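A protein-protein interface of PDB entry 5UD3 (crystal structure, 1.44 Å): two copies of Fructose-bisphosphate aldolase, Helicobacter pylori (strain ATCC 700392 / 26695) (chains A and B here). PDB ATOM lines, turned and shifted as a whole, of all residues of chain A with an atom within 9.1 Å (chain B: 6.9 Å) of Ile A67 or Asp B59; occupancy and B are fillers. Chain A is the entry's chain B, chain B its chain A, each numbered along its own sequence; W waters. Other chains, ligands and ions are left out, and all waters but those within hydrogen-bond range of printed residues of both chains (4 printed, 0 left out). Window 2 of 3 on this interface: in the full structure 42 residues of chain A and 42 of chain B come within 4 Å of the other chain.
Asn A31 touches none of the printed residues of chain B.
Printed residues of chain B within 4 Å of Asp A59: Ile B67 (3.8 Å).
Of the printed residues of chain B, Gly A63 touches Ile B67.
Of the printed residues of chain B, Met A64 touches Met B60 (3.7 Å) and Met B64 (3.9 Å).
Ile A67 touches just these residues of chain B: Asp B59, Met B60 and Gly B63.
Of chain A, only Ile A67 (3.7 Å) and Arg A71 (2.9 Å) come within 4 Å of Asp B59.
Of the printed residues of chain A, Met B60 touches Phe A27, Met A64, Ile A67, Met A68 and Arg A71.
Gly B63 touches just one residue of chain A: Ile A67 (3.6 Å).
The nearest printed residue of chain A that does not touch Met B64 is Ile A67 (4.2 Å).
NH1 of Arg A71 is in hydrogen-bond range of OD1 of Asn A31 (3.3 Å).
The guanidinium group (NH1) of Arg A71 sits at hydrogen-bond distance from the side-chain sulfur (SD) of Met A68 (3.8 Å).
Asp A59 touches Ile B67, and with the chains exchanged Ile A67 touches Asp B59.
Met A60 touches Ile B67, and with the chains exchanged Ile A67 touches Met B60.
Gly A63 touches Ile B67, and with the chains exchanged Ile A67 touches Gly B63.
Met B64 touches its own counterpart, Met A64.
Positions printed for both chains: 59, 60, 61, 62, 63, 64 and 67.
Of the 16 pairs that touch across the chains among the printed residues, 9 have their exchanged pair printed and touching as well.
O of Met B56 is in hydrogen-bond range of NH2 of Arg A71.
The side-chain carboxylate (OD2) of Asp B59 is in salt-bridge range of the guanidinium group (NH2) of Arg A71, 2.9 Å away.
Hydrophobic or aromatic side chains of chain B that line the printed part of chain A: Met B60, Met B64 and Ile B67.
Water W3 lies within hydrogen-bond range of the side-chain carboxylate (OD1) of Asp B59 (2.6 Å) and the backbone carbonyl oxygen (O) of Ile A67 (2.8 Å).
Water W2 bridges the side-chain carboxylate (OD1) of Asp A59 and the backbone carbonyl oxygen (O) of Ile B67.
Water W1 bridges OD2 of Asp B59 and NE of Arg A71.
Water W4 bridges the guanidinium group (NH1) of Arg A71 (3.1 Å) and the backbone carbonyl oxygen (O) of Met B56 (3.3 Å).
Phe A27 touches Met B56 (CZ to O, 3.6 Å).
Asp A59 touches Ile B67.
Met A60 touches Met B64.
Met A60 touches Ile B67.
Met A64 touches Met B60 (O to CE, 3.7 Å).
Asp B59 touches Ile A67 (OD1 to CG2, 3.7 Å).
CD1 of Ile A67 touches CA of Gly B63, 3.6 Å away.
Met A68 touches Met B60 (SD to CE, 3.5 Å).
NH2 of Arg A71 touches CA of Gly B57, 3.7 Å away.
CB of Met B60 touches NH2 of Arg A71, 3.5 Å away.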
ATOM      1  N   LEU A   2     -24.997 -11.500   9.624  1.00  0.00           N
ATOM      2  CA  LEU A   2     -25.230 -11.840  11.027  1.00  0.00           C
ATOM      3  C   LEU A   2     -26.617 -11.371  11.465  1.00  0.00           C
ATOM      4  O   LEU A   2     -26.925 -10.177  11.381  1.00  0.00           O
ATOM      5  CB  LEU A   2     -24.164 -11.153  11.866  1.00  0.00           C
ATOM      6  CG  LEU A   2     -24.127 -11.499  13.352  1.00  0.00           C
ATOM      7  CD1 LEU A   2     -23.996 -12.997  13.592  1.00  0.00           C
ATOM      8  CD2 LEU A   2     -22.951 -10.788  13.977  1.00  0.00           C
ATOM      9  N   PHE A  27      -9.842 -20.054  15.320  1.00  0.00           N
ATOM     10  CA  PHE A  27     -10.014 -19.690  13.917  1.00  0.00           C
ATOM     11  C   PHE A  27     -10.242 -20.916  13.042  1.00  0.00           C
ATOM     12  O   PHE A  27     -11.097 -20.905  12.153  1.00  0.00           O
ATOM     13  CB  PHE A  27      -8.784 -18.935  13.398  1.00  0.00           C
ATOM     14  CG  PHE A  27      -8.720 -18.888  11.899  1.00  0.00           C
ATOM     15  CD1 PHE A  27      -9.619 -18.122  11.181  1.00  0.00           C
ATOM     16  CD2 PHE A  27      -7.795 -19.646  11.207  1.00  0.00           C
ATOM     17  CE1 PHE A  27      -9.591 -18.099   9.808  1.00  0.00           C
ATOM     18  CE2 PHE A  27      -7.765 -19.627   9.822  1.00  0.00           C
ATOM     19  CZ  PHE A  27      -8.666 -18.856   9.128  1.00  0.00           C
ATOM     20  N   LEU A  30     -13.725 -22.270  13.184  1.00  0.00           N
ATOM     21  CA  LEU A  30     -14.665 -21.326  12.601  1.00  0.00           C
ATOM     22  C   LEU A  30     -14.559 -21.307  11.086  1.00  0.00           C
ATOM     23  O   LEU A  30     -15.576 -21.269  10.387  1.00  0.00           O
ATOM     24  CB  LEU A  30     -14.398 -19.940  13.171  1.00  0.00           C
ATOM     25  CG  LEU A  30     -15.379 -18.841  12.810  1.00  0.00           C
ATOM     26  CD1 LEU A  30     -16.739 -19.123  13.434  1.00  0.00           C
ATOM     27  CD2 LEU A  30     -14.821 -17.521  13.294  1.00  0.00           C
ATOM     28  N   ASN A  31     -13.333 -21.309  10.555  1.00  0.00           N
ATOM     29  CA  ASN A  31     -13.166 -21.262   9.108  1.00  0.00           C
ATOM     30  C   ASN A  31     -13.777 -22.487   8.448  1.00  0.00           C
ATOM     31  O   ASN A  31     -14.463 -22.373   7.428  1.00  0.00           O
ATOM     32  CB  ASN A  31     -11.687 -21.157   8.765  1.00  0.00           C
ATOM     33  CG  ASN A  31     -11.456 -20.839   7.300  1.00  0.00           C
ATOM     34  OD1 ASN A  31     -12.090 -19.946   6.737  1.00  0.00           O
ATOM     35  ND2 ASN A  31     -10.566 -21.584   6.677  1.00  0.00           N
ATOM     36  N   PHE A  34     -17.650 -22.252   8.356  1.00  0.00           N
ATOM     37  CA  PHE A  34     -18.136 -21.327   7.334  1.00  0.00           C
ATOM     38  C   PHE A  34     -17.932 -21.882   5.928  1.00  0.00           C
ATOM     39  O   PHE A  34     -18.818 -21.760   5.077  1.00  0.00           O
ATOM     40  CB  PHE A  34     -17.440 -19.975   7.469  1.00  0.00           C
ATOM     41  CG  PHE A  34     -18.175 -18.999   8.341  1.00  0.00           C
ATOM     42  CD1 PHE A  34     -18.052 -19.046   9.719  1.00  0.00           C
ATOM     43  CD2 PHE A  34     -18.991 -18.032   7.777  1.00  0.00           C
ATOM     44  CE1 PHE A  34     -18.735 -18.139  10.517  1.00  0.00           C
ATOM     45  CE2 PHE A  34     -19.671 -17.124   8.564  1.00  0.00           C
ATOM     46  CZ  PHE A  34     -19.542 -17.178   9.931  1.00  0.00           C
ATOM     47  N   ASP A  59     -14.276 -10.653  22.956  1.00  0.00           N
ATOM     48  CA  ASP A  59     -13.993  -9.716  21.869  1.00  0.00           C
ATOM     49  C   ASP A  59     -13.483 -10.439  20.626  1.00  0.00           C
ATOM     50  O   ASP A  59     -13.805 -10.054  19.493  1.00  0.00           O
ATOM     51  CB  ASP A  59     -12.986  -8.653  22.343  1.00  0.00           C
ATOM     52  CG  ASP A  59     -11.716  -9.247  22.999  1.00  0.00           C
ATOM     53  OD1 ASP A  59     -10.641  -8.612  22.913  1.00  0.00           O
ATOM     54  OD2 ASP A  59     -11.783 -10.327  23.624  1.00  0.00           O
ATOM     55  N   MET A  60     -12.671 -11.478  20.816  1.00  0.00           N
ATOM     56  CA  MET A  60     -12.160 -12.235  19.682  1.00  0.00           C
ATOM     57  C   MET A  60     -13.212 -13.186  19.129  1.00  0.00           C
ATOM     58  O   MET A  60     -13.310 -13.366  17.907  1.00  0.00           O
ATOM     59  CB  MET A  60     -10.899 -12.999  20.092  1.00  0.00           C
ATOM     60  CG  MET A  60     -10.226 -13.737  18.943  1.00  0.00           C
ATOM     61  SD  MET A  60      -9.569 -12.646  17.652  1.00  0.00           S
ATOM     62  CE  MET A  60      -8.136 -11.959  18.497  1.00  0.00           C
ATOM     63  N   ALA A  61     -14.020 -13.788  20.010  1.00  0.00           N
ATOM     64  CA  ALA A  61     -15.094 -14.664  19.555  1.00  0.00           C
ATOM     65  C   ALA A  61     -16.024 -13.915  18.614  1.00  0.00           C
ATOM     66  O   ALA A  61     -16.279 -14.358  17.487  1.00  0.00           O
ATOM     67  CB  ALA A  61     -15.871 -15.210  20.753  1.00  0.00           C
ATOM     68  N   VAL A  62     -16.515 -12.754  19.051  1.00  0.00           N
ATOM     69  CA  VAL A  62     -17.406 -11.964  18.209  1.00  0.00           C
ATOM     70  C   VAL A  62     -16.662 -11.425  17.005  1.00  0.00           C
ATOM     71  O   VAL A  62     -17.173 -11.464  15.879  1.00  0.00           O
ATOM     72  CB  VAL A  62     -18.049 -10.833  19.022  1.00  0.00           C
ATOM     73  CG1 VAL A  62     -18.923  -9.979  18.125  1.00  0.00           C
ATOM     74  CG2 VAL A  62     -18.858 -11.406  20.166  1.00  0.00           C
ATOM     75  N   GLY A  63     -15.448 -10.912  17.218  1.00  0.00           N
ATOM     76  CA  GLY A  63     -14.738 -10.258  16.134  1.00  0.00           C
ATOM     77  C   GLY A  63     -14.406 -11.196  14.989  1.00  0.00           C
ATOM     78  O   GLY A  63     -14.511 -10.819  13.821  1.00  0.00           O
ATOM     79  N   MET A  64     -13.961 -12.415  15.303  1.00  0.00           N
ATOM     80  CA  MET A  64     -13.674 -13.380  14.246  1.00  0.00           C
ATOM     81  C   MET A  64     -14.938 -13.734  13.476  1.00  0.00           C
ATOM     82  O   MET A  64     -14.912 -13.844  12.242  1.00  0.00           O
ATOM     83  CB  MET A  64     -13.028 -14.645  14.812  1.00  0.00           C
ATOM     84  CG  MET A  64     -11.564 -14.477  15.225  1.00  0.00           C
ATOM     85  SD  MET A  64     -10.700 -16.043  15.489  1.00  0.00           S
ATOM     86  CE  MET A  64     -11.820 -16.825  16.622  1.00  0.00           C
ATOM     87  N   VAL A  65     -16.061 -13.914  14.181  1.00  0.00           N
ATOM     88  CA  VAL A  65     -17.300 -14.248  13.492  1.00  0.00           C
ATOM     89  C   VAL A  65     -17.726 -13.107  12.577  1.00  0.00           C
ATOM     90  O   VAL A  65     -18.174 -13.336  11.451  1.00  0.00           O
ATOM     91  CB  VAL A  65     -18.400 -14.637  14.498  1.00  0.00           C
ATOM     92  CG1 VAL A  65     -19.742 -14.820  13.787  1.00  0.00           C
ATOM     93  CG2 VAL A  65     -18.011 -15.896  15.224  1.00  0.00           C
ATOM     94  N   LYS A  66     -17.584 -11.863  13.033  1.00  0.00           N
ATOM     95  CA  LYS A  66     -17.960 -10.740  12.183  1.00  0.00           C
ATOM     96  C   LYS A  66     -17.102 -10.686  10.926  1.00  0.00           C
ATOM     97  O   LYS A  66     -17.606 -10.386   9.840  1.00  0.00           O
ATOM     98  CB  LYS A  66     -17.918  -9.432  12.972  1.00  0.00           C
ATOM     99  CG  LYS A  66     -19.089  -9.334  13.960  1.00  0.00           C
ATOM    100  CD  LYS A  66     -19.227  -7.974  14.619  1.00  0.00           C
ATOM    101  CE  LYS A  66     -20.497  -7.917  15.473  1.00  0.00           C
ATOM    102  NZ  LYS A  66     -20.577  -6.661  16.272  1.00  0.00           N
ATOM    103  N   ILE A  67     -15.812 -11.007  11.043  1.00  0.00           N
ATOM    104  CA  ILE A  67     -14.960 -11.051   9.855  1.00  0.00           C
ATOM    105  C   ILE A  67     -15.450 -12.129   8.898  1.00  0.00           C
ATOM    106  O   ILE A  67     -15.522 -11.920   7.682  1.00  0.00           O
ATOM    107  CB  ILE A  67     -13.494 -11.278  10.263  1.00  0.00           C
ATOM    108  CG1 ILE A  67     -12.953 -10.041  10.980  1.00  0.00           C
ATOM    109  CG2 ILE A  67     -12.629 -11.569   9.041  1.00  0.00           C
ATOM    110  CD1 ILE A  67     -11.745 -10.303  11.837  1.00  0.00           C
ATOM    111  N   MET A  68     -15.802 -13.298   9.432  1.00  0.00           N
ATOM    112  CA  MET A  68     -16.235 -14.398   8.574  1.00  0.00           C
ATOM    113  C   MET A  68     -17.568 -14.090   7.905  1.00  0.00           C
ATOM    114  O   MET A  68     -17.782 -14.451   6.743  1.00  0.00           O
ATOM    115  CB  MET A  68     -16.326 -15.693   9.385  1.00  0.00           C
ATOM    116  CG  MET A  68     -14.975 -16.204   9.892  1.00  0.00           C
ATOM    117  SD  MET A  68     -13.753 -16.492   8.569  1.00  0.00           S
ATOM    118  CE  MET A  68     -14.575 -17.767   7.656  1.00  0.00           C
ATOM    119  N   CYS A  69     -18.477 -13.438   8.632  1.00  0.00           N
ATOM    120  CA  CYS A  69     -19.745 -13.031   8.039  1.00  0.00           C
ATOM    121  C   CYS A  69     -19.524 -12.065   6.878  1.00  0.00           C
ATOM    122  O   CYS A  69     -20.188 -12.171   5.839  1.00  0.00           O
ATOM    123  CB  CYS A  69     -20.642 -12.415   9.113  1.00  0.00           C
ATOM    124  SG  CYS A  69     -21.336 -13.632  10.257  1.00  0.00           S
ATOM    125  N   GLU A  70     -18.585 -11.125   7.028  1.00  0.00           N
ATOM    126  CA  GLU A  70     -18.272 -10.205   5.937  1.00  0.00           C
ATOM    127  C   GLU A  70     -17.613 -10.924   4.768  1.00  0.00           C
ATOM    128  O   GLU A  70     -17.747 -10.490   3.618  1.00  0.00           O
ATOM    129  CB  GLU A  70     -17.375  -9.073   6.444  1.00  0.00           C
ATOM    130  CG  GLU A  70     -18.071  -8.129   7.419  1.00  0.00           C
ATOM    131  CD  GLU A  70     -17.138  -7.084   7.997  1.00  0.00           C
ATOM    132  OE1 GLU A  70     -17.400  -6.611   9.124  1.00  0.00           O
ATOM    133  OE2 GLU A  70     -16.143  -6.735   7.327  1.00  0.00           O
ATOM    134  N   ARG A  71     -16.906 -12.021   5.039  1.00  0.00           N
ATOM    135  CA  ARG A  71     -16.293 -12.807   3.977  1.00  0.00           C
ATOM    136  C   ARG A  71     -17.338 -13.584   3.188  1.00  0.00           C
ATOM    137  O   ARG A  71     -17.164 -13.807   1.984  1.00  0.00           O
ATOM    138  CB  ARG A  71     -15.271 -13.747   4.615  1.00  0.00           C
ATOM    139  CG  ARG A  71     -14.426 -14.528   3.659  1.00  0.00           C
ATOM    140  CD  ARG A  71     -13.537 -15.509   4.382  1.00  0.00           C
ATOM    141  NE  ARG A  71     -12.414 -14.869   5.064  1.00  0.00           N
ATOM    142  CZ  ARG A  71     -11.425 -15.539   5.647  1.00  0.00           C
ATOM    143  NH1 ARG A  71     -11.415 -16.868   5.633  1.00  0.00           N
ATOM    144  NH2 ARG A  71     -10.437 -14.882   6.243  1.00  0.00           N
ATOM    145  N   TYR A  72     -18.435 -13.978   3.839  1.00  0.00           N
ATOM    146  CA  TYR A  72     -19.509 -14.760   3.225  1.00  0.00           C
ATOM    147  C   TYR A  72     -20.837 -14.067   3.518  1.00  0.00           C
ATOM    148  O   TYR A  72     -21.665 -14.578   4.282  1.00  0.00           O
ATOM    149  CB  TYR A  72     -19.526 -16.184   3.778  1.00  0.00           C
ATOM    150  CG  TYR A  72     -18.290 -16.994   3.486  1.00  0.00           C
ATOM    151  CD1 TYR A  72     -17.324 -17.203   4.459  1.00  0.00           C
ATOM    152  CD2 TYR A  72     -18.090 -17.549   2.236  1.00  0.00           C
ATOM    153  CE1 TYR A  72     -16.189 -17.945   4.192  1.00  0.00           C
ATOM    154  CE2 TYR A  72     -16.959 -18.293   1.956  1.00  0.00           C
ATOM    155  CZ  TYR A  72     -16.008 -18.483   2.939  1.00  0.00           C
ATOM    156  OH  TYR A  72     -14.879 -19.227   2.662  1.00  0.00           O
ATOM    157  N   PRO A  73     -21.073 -12.894   2.928  1.00  0.00           N
ATOM    158  CA  PRO A  73     -22.244 -12.094   3.333  1.00  0.00           C
ATOM    159  C   PRO A  73     -23.584 -12.704   2.956  1.00  0.00           C
ATOM    160  O   PRO A  73     -24.610 -12.301   3.519  1.00  0.00           O
ATOM    161  CB  PRO A  73     -22.011 -10.749   2.634  1.00  0.00           C
ATOM    162  CG  PRO A  73     -21.102 -11.077   1.479  1.00  0.00           C
ATOM    163  CD  PRO A  73     -20.218 -12.189   1.954  1.00  0.00           C
ATOM    164  N   LEU A  79     -24.923 -15.871  15.900  1.00  0.00           N
ATOM    165  CA  LEU A  79     -23.841 -16.090  16.851  1.00  0.00           C
ATOM    166  C   LEU A  79     -24.467 -16.276  18.231  1.00  0.00           C
ATOM    167  O   LEU A  79     -25.104 -15.358  18.755  1.00  0.00           O
ATOM    168  CB  LEU A  79     -22.884 -14.904  16.859  1.00  0.00           C
ATOM    169  CG  LEU A  79     -21.798 -14.978  17.926  1.00  0.00           C
ATOM    170  CD1 LEU A  79     -21.038 -16.289  17.858  1.00  0.00           C
ATOM    171  CD2 LEU A  79     -20.860 -13.808  17.766  1.00  0.00           C
ATOM    172  N   ILE B  53      -0.824 -15.423   5.233  1.00  0.00           N
ATOM    173  CA  ILE B  53      -1.953 -14.635   4.751  1.00  0.00           C
ATOM    174  C   ILE B  53      -2.901 -15.497   3.929  1.00  0.00           C
ATOM    175  O   ILE B  53      -4.127 -15.359   4.027  1.00  0.00           O
ATOM    176  CB  ILE B  53      -1.457 -13.399   3.973  1.00  0.00           C
ATOM    177  CG1 ILE B  53      -0.871 -12.376   4.950  1.00  0.00           C
ATOM    178  CG2 ILE B  53      -2.586 -12.748   3.182  1.00  0.00           C
ATOM    179  CD1 ILE B  53      -0.074 -11.289   4.267  1.00  0.00           C
ATOM    180  N   MET B  56      -4.872 -17.706   6.553  1.00  0.00           N
ATOM    181  CA  MET B  56      -5.861 -17.007   7.371  1.00  0.00           C
ATOM    182  C   MET B  56      -6.866 -16.234   6.537  1.00  0.00           C
ATOM    183  O   MET B  56      -8.014 -16.061   6.964  1.00  0.00           O
ATOM    184  CB  MET B  56      -5.160 -15.986   8.270  1.00  0.00           C
ATOM    185  CG  MET B  56      -4.421 -16.580   9.456  1.00  0.00           C
ATOM    186  SD  MET B  56      -3.623 -15.339  10.498  1.00  0.00           S
ATOM    187  CE  MET B  56      -2.122 -14.998   9.563  1.00  0.00           C
ATOM    188  N   GLY B  57      -6.457 -15.762   5.363  1.00  0.00           N
ATOM    189  CA  GLY B  57      -7.137 -14.691   4.661  1.00  0.00           C
ATOM    190  C   GLY B  57      -6.662 -13.360   5.198  1.00  0.00           C
ATOM    191  O   GLY B  57      -6.571 -13.189   6.413  1.00  0.00           O
ATOM    192  N   ILE B  58      -6.327 -12.417   4.312  1.00  0.00           N
ATOM    193  CA  ILE B  58      -5.741 -11.161   4.770  1.00  0.00           C
ATOM    194  C   ILE B  58      -6.709 -10.394   5.664  1.00  0.00           C
ATOM    195  O   ILE B  58      -6.282  -9.674   6.575  1.00  0.00           O
ATOM    196  CB  ILE B  58      -5.256 -10.323   3.568  1.00  0.00           C
ATOM    197  CG1 ILE B  58      -4.198  -9.317   4.023  1.00  0.00           C
ATOM    198  CG2 ILE B  58      -6.428  -9.616   2.887  1.00  0.00           C
ATOM    199  CD1 ILE B  58      -3.422  -8.702   2.873  1.00  0.00           C
ATOM    200  N   ASP B  59      -8.017 -10.524   5.416  1.00  0.00           N
ATOM    201  CA  ASP B  59      -9.025  -9.889   6.261  1.00  0.00           C
ATOM    202  C   ASP B  59      -8.972 -10.401   7.696  1.00  0.00           C
ATOM    203  O   ASP B  59      -9.177  -9.635   8.644  1.00  0.00           O
ATOM    204  CB  ASP B  59     -10.422 -10.103   5.657  1.00  0.00           C
ATOM    205  CG  ASP B  59     -10.749 -11.585   5.355  1.00  0.00           C
ATOM    206  OD1 ASP B  59     -11.937 -11.962   5.450  1.00  0.00           O
ATOM    207  OD2 ASP B  59      -9.849 -12.377   5.001  1.00  0.00           O
ATOM    208  N   MET B  60      -8.709 -11.695   7.879  1.00  0.00           N
ATOM    209  CA  MET B  60      -8.625 -12.245   9.230  1.00  0.00           C
ATOM    210  C   MET B  60      -7.283 -11.926   9.880  1.00  0.00           C
ATOM    211  O   MET B  60      -7.220 -11.671  11.089  1.00  0.00           O
ATOM    212  CB  MET B  60      -8.870 -13.749   9.185  1.00  0.00           C
ATOM    213  CG  MET B  60      -8.894 -14.409  10.536  1.00  0.00           C
ATOM    214  SD  MET B  60     -10.276 -13.904  11.594  1.00  0.00           S
ATOM    215  CE  MET B  60     -11.644 -14.755  10.808  1.00  0.00           C
ATOM    216  N   ALA B  61      -6.197 -11.948   9.099  1.00  0.00           N
ATOM    217  CA  ALA B  61      -4.892 -11.580   9.632  1.00  0.00           C
ATOM    218  C   ALA B  61      -4.943 -10.189  10.243  1.00  0.00           C
ATOM    219  O   ALA B  61      -4.589  -9.998  11.415  1.00  0.00           O
ATOM    220  CB  ALA B  61      -3.836 -11.656   8.523  1.00  0.00           C
ATOM    221  N   VAL B  62      -5.408  -9.203   9.470  1.00  0.00           N
ATOM    222  CA  VAL B  62      -5.496  -7.843   9.985  1.00  0.00           C
ATOM    223  C   VAL B  62      -6.537  -7.757  11.087  1.00  0.00           C
ATOM    224  O   VAL B  62      -6.310  -7.130  12.129  1.00  0.00           O
ATOM    225  CB  VAL B  62      -5.815  -6.860   8.851  1.00  0.00           C
ATOM    226  CG1 VAL B  62      -6.022  -5.453   9.413  1.00  0.00           C
ATOM    227  CG2 VAL B  62      -4.714  -6.876   7.804  1.00  0.00           C
ATOM    228  N   GLY B  63      -7.699  -8.380  10.875  1.00  0.00           N
ATOM    229  CA  GLY B  63      -8.789  -8.237  11.827  1.00  0.00           C
ATOM    230  C   GLY B  63      -8.448  -8.767  13.206  1.00  0.00           C
ATOM    231  O   GLY B  63      -8.794  -8.149  14.213  1.00  0.00           O
ATOM    232  N   MET B  64      -7.790  -9.930  13.271  1.00  0.00           N
ATOM    233  CA  MET B  64      -7.398 -10.482  14.564  1.00  0.00           C
ATOM    234  C   MET B  64      -6.394  -9.574  15.249  1.00  0.00           C
ATOM    235  O   MET B  64      -6.467  -9.359  16.459  1.00  0.00           O
ATOM    236  CB  MET B  64      -6.820 -11.891  14.422  1.00  0.00           C
ATOM    237  CG  MET B  64      -7.849 -12.976  14.098  1.00  0.00           C
ATOM    238  SD  MET B  64      -7.274 -14.680  14.361  1.00  0.00           S
ATOM    239  CE  MET B  64      -5.852 -14.706  13.290  1.00  0.00           C
ATOM    240  N   ILE B  67      -8.135  -6.583  16.802  1.00  0.00           N
ATOM    241  CA  ILE B  67      -8.792  -6.972  18.049  1.00  0.00           C
ATOM    242  C   ILE B  67      -7.779  -7.035  19.181  1.00  0.00           C
ATOM    243  O   ILE B  67      -8.022  -6.545  20.291  1.00  0.00           O
ATOM    244  CB  ILE B  67      -9.520  -8.316  17.866  1.00  0.00           C
ATOM    245  CG1 ILE B  67     -10.722  -8.125  16.938  1.00  0.00           C
ATOM    246  CG2 ILE B  67      -9.981  -8.874  19.217  1.00  0.00           C
ATOM    247  CD1 ILE B  67     -11.189  -9.390  16.269  1.00  0.00           C
ATOM    248  N   ALA B  96      -5.121  -3.559   2.915  1.00  0.00           N
ATOM    249  CA  ALA B  96      -5.820  -4.292   3.959  1.00  0.00           C
ATOM    250  C   ALA B  96      -5.575  -3.721   5.350  1.00  0.00           C
ATOM    251  O   ALA B  96      -6.353  -4.021   6.267  1.00  0.00           O
ATOM    252  CB  ALA B  96      -5.409  -5.761   3.927  1.00  0.00           C
HETATM  253  O   HOH W   1     -10.106 -13.942   2.722  1.00  0.00           O
HETATM  254  O   HOH W   2     -10.411  -6.236  21.691  1.00  0.00           O
HETATM  255  O   HOH W   3     -13.966 -10.363   5.981  1.00  0.00           O
HETATM  256  O   HOH W   4      -8.868 -18.627   5.146  1.00  0.00           O
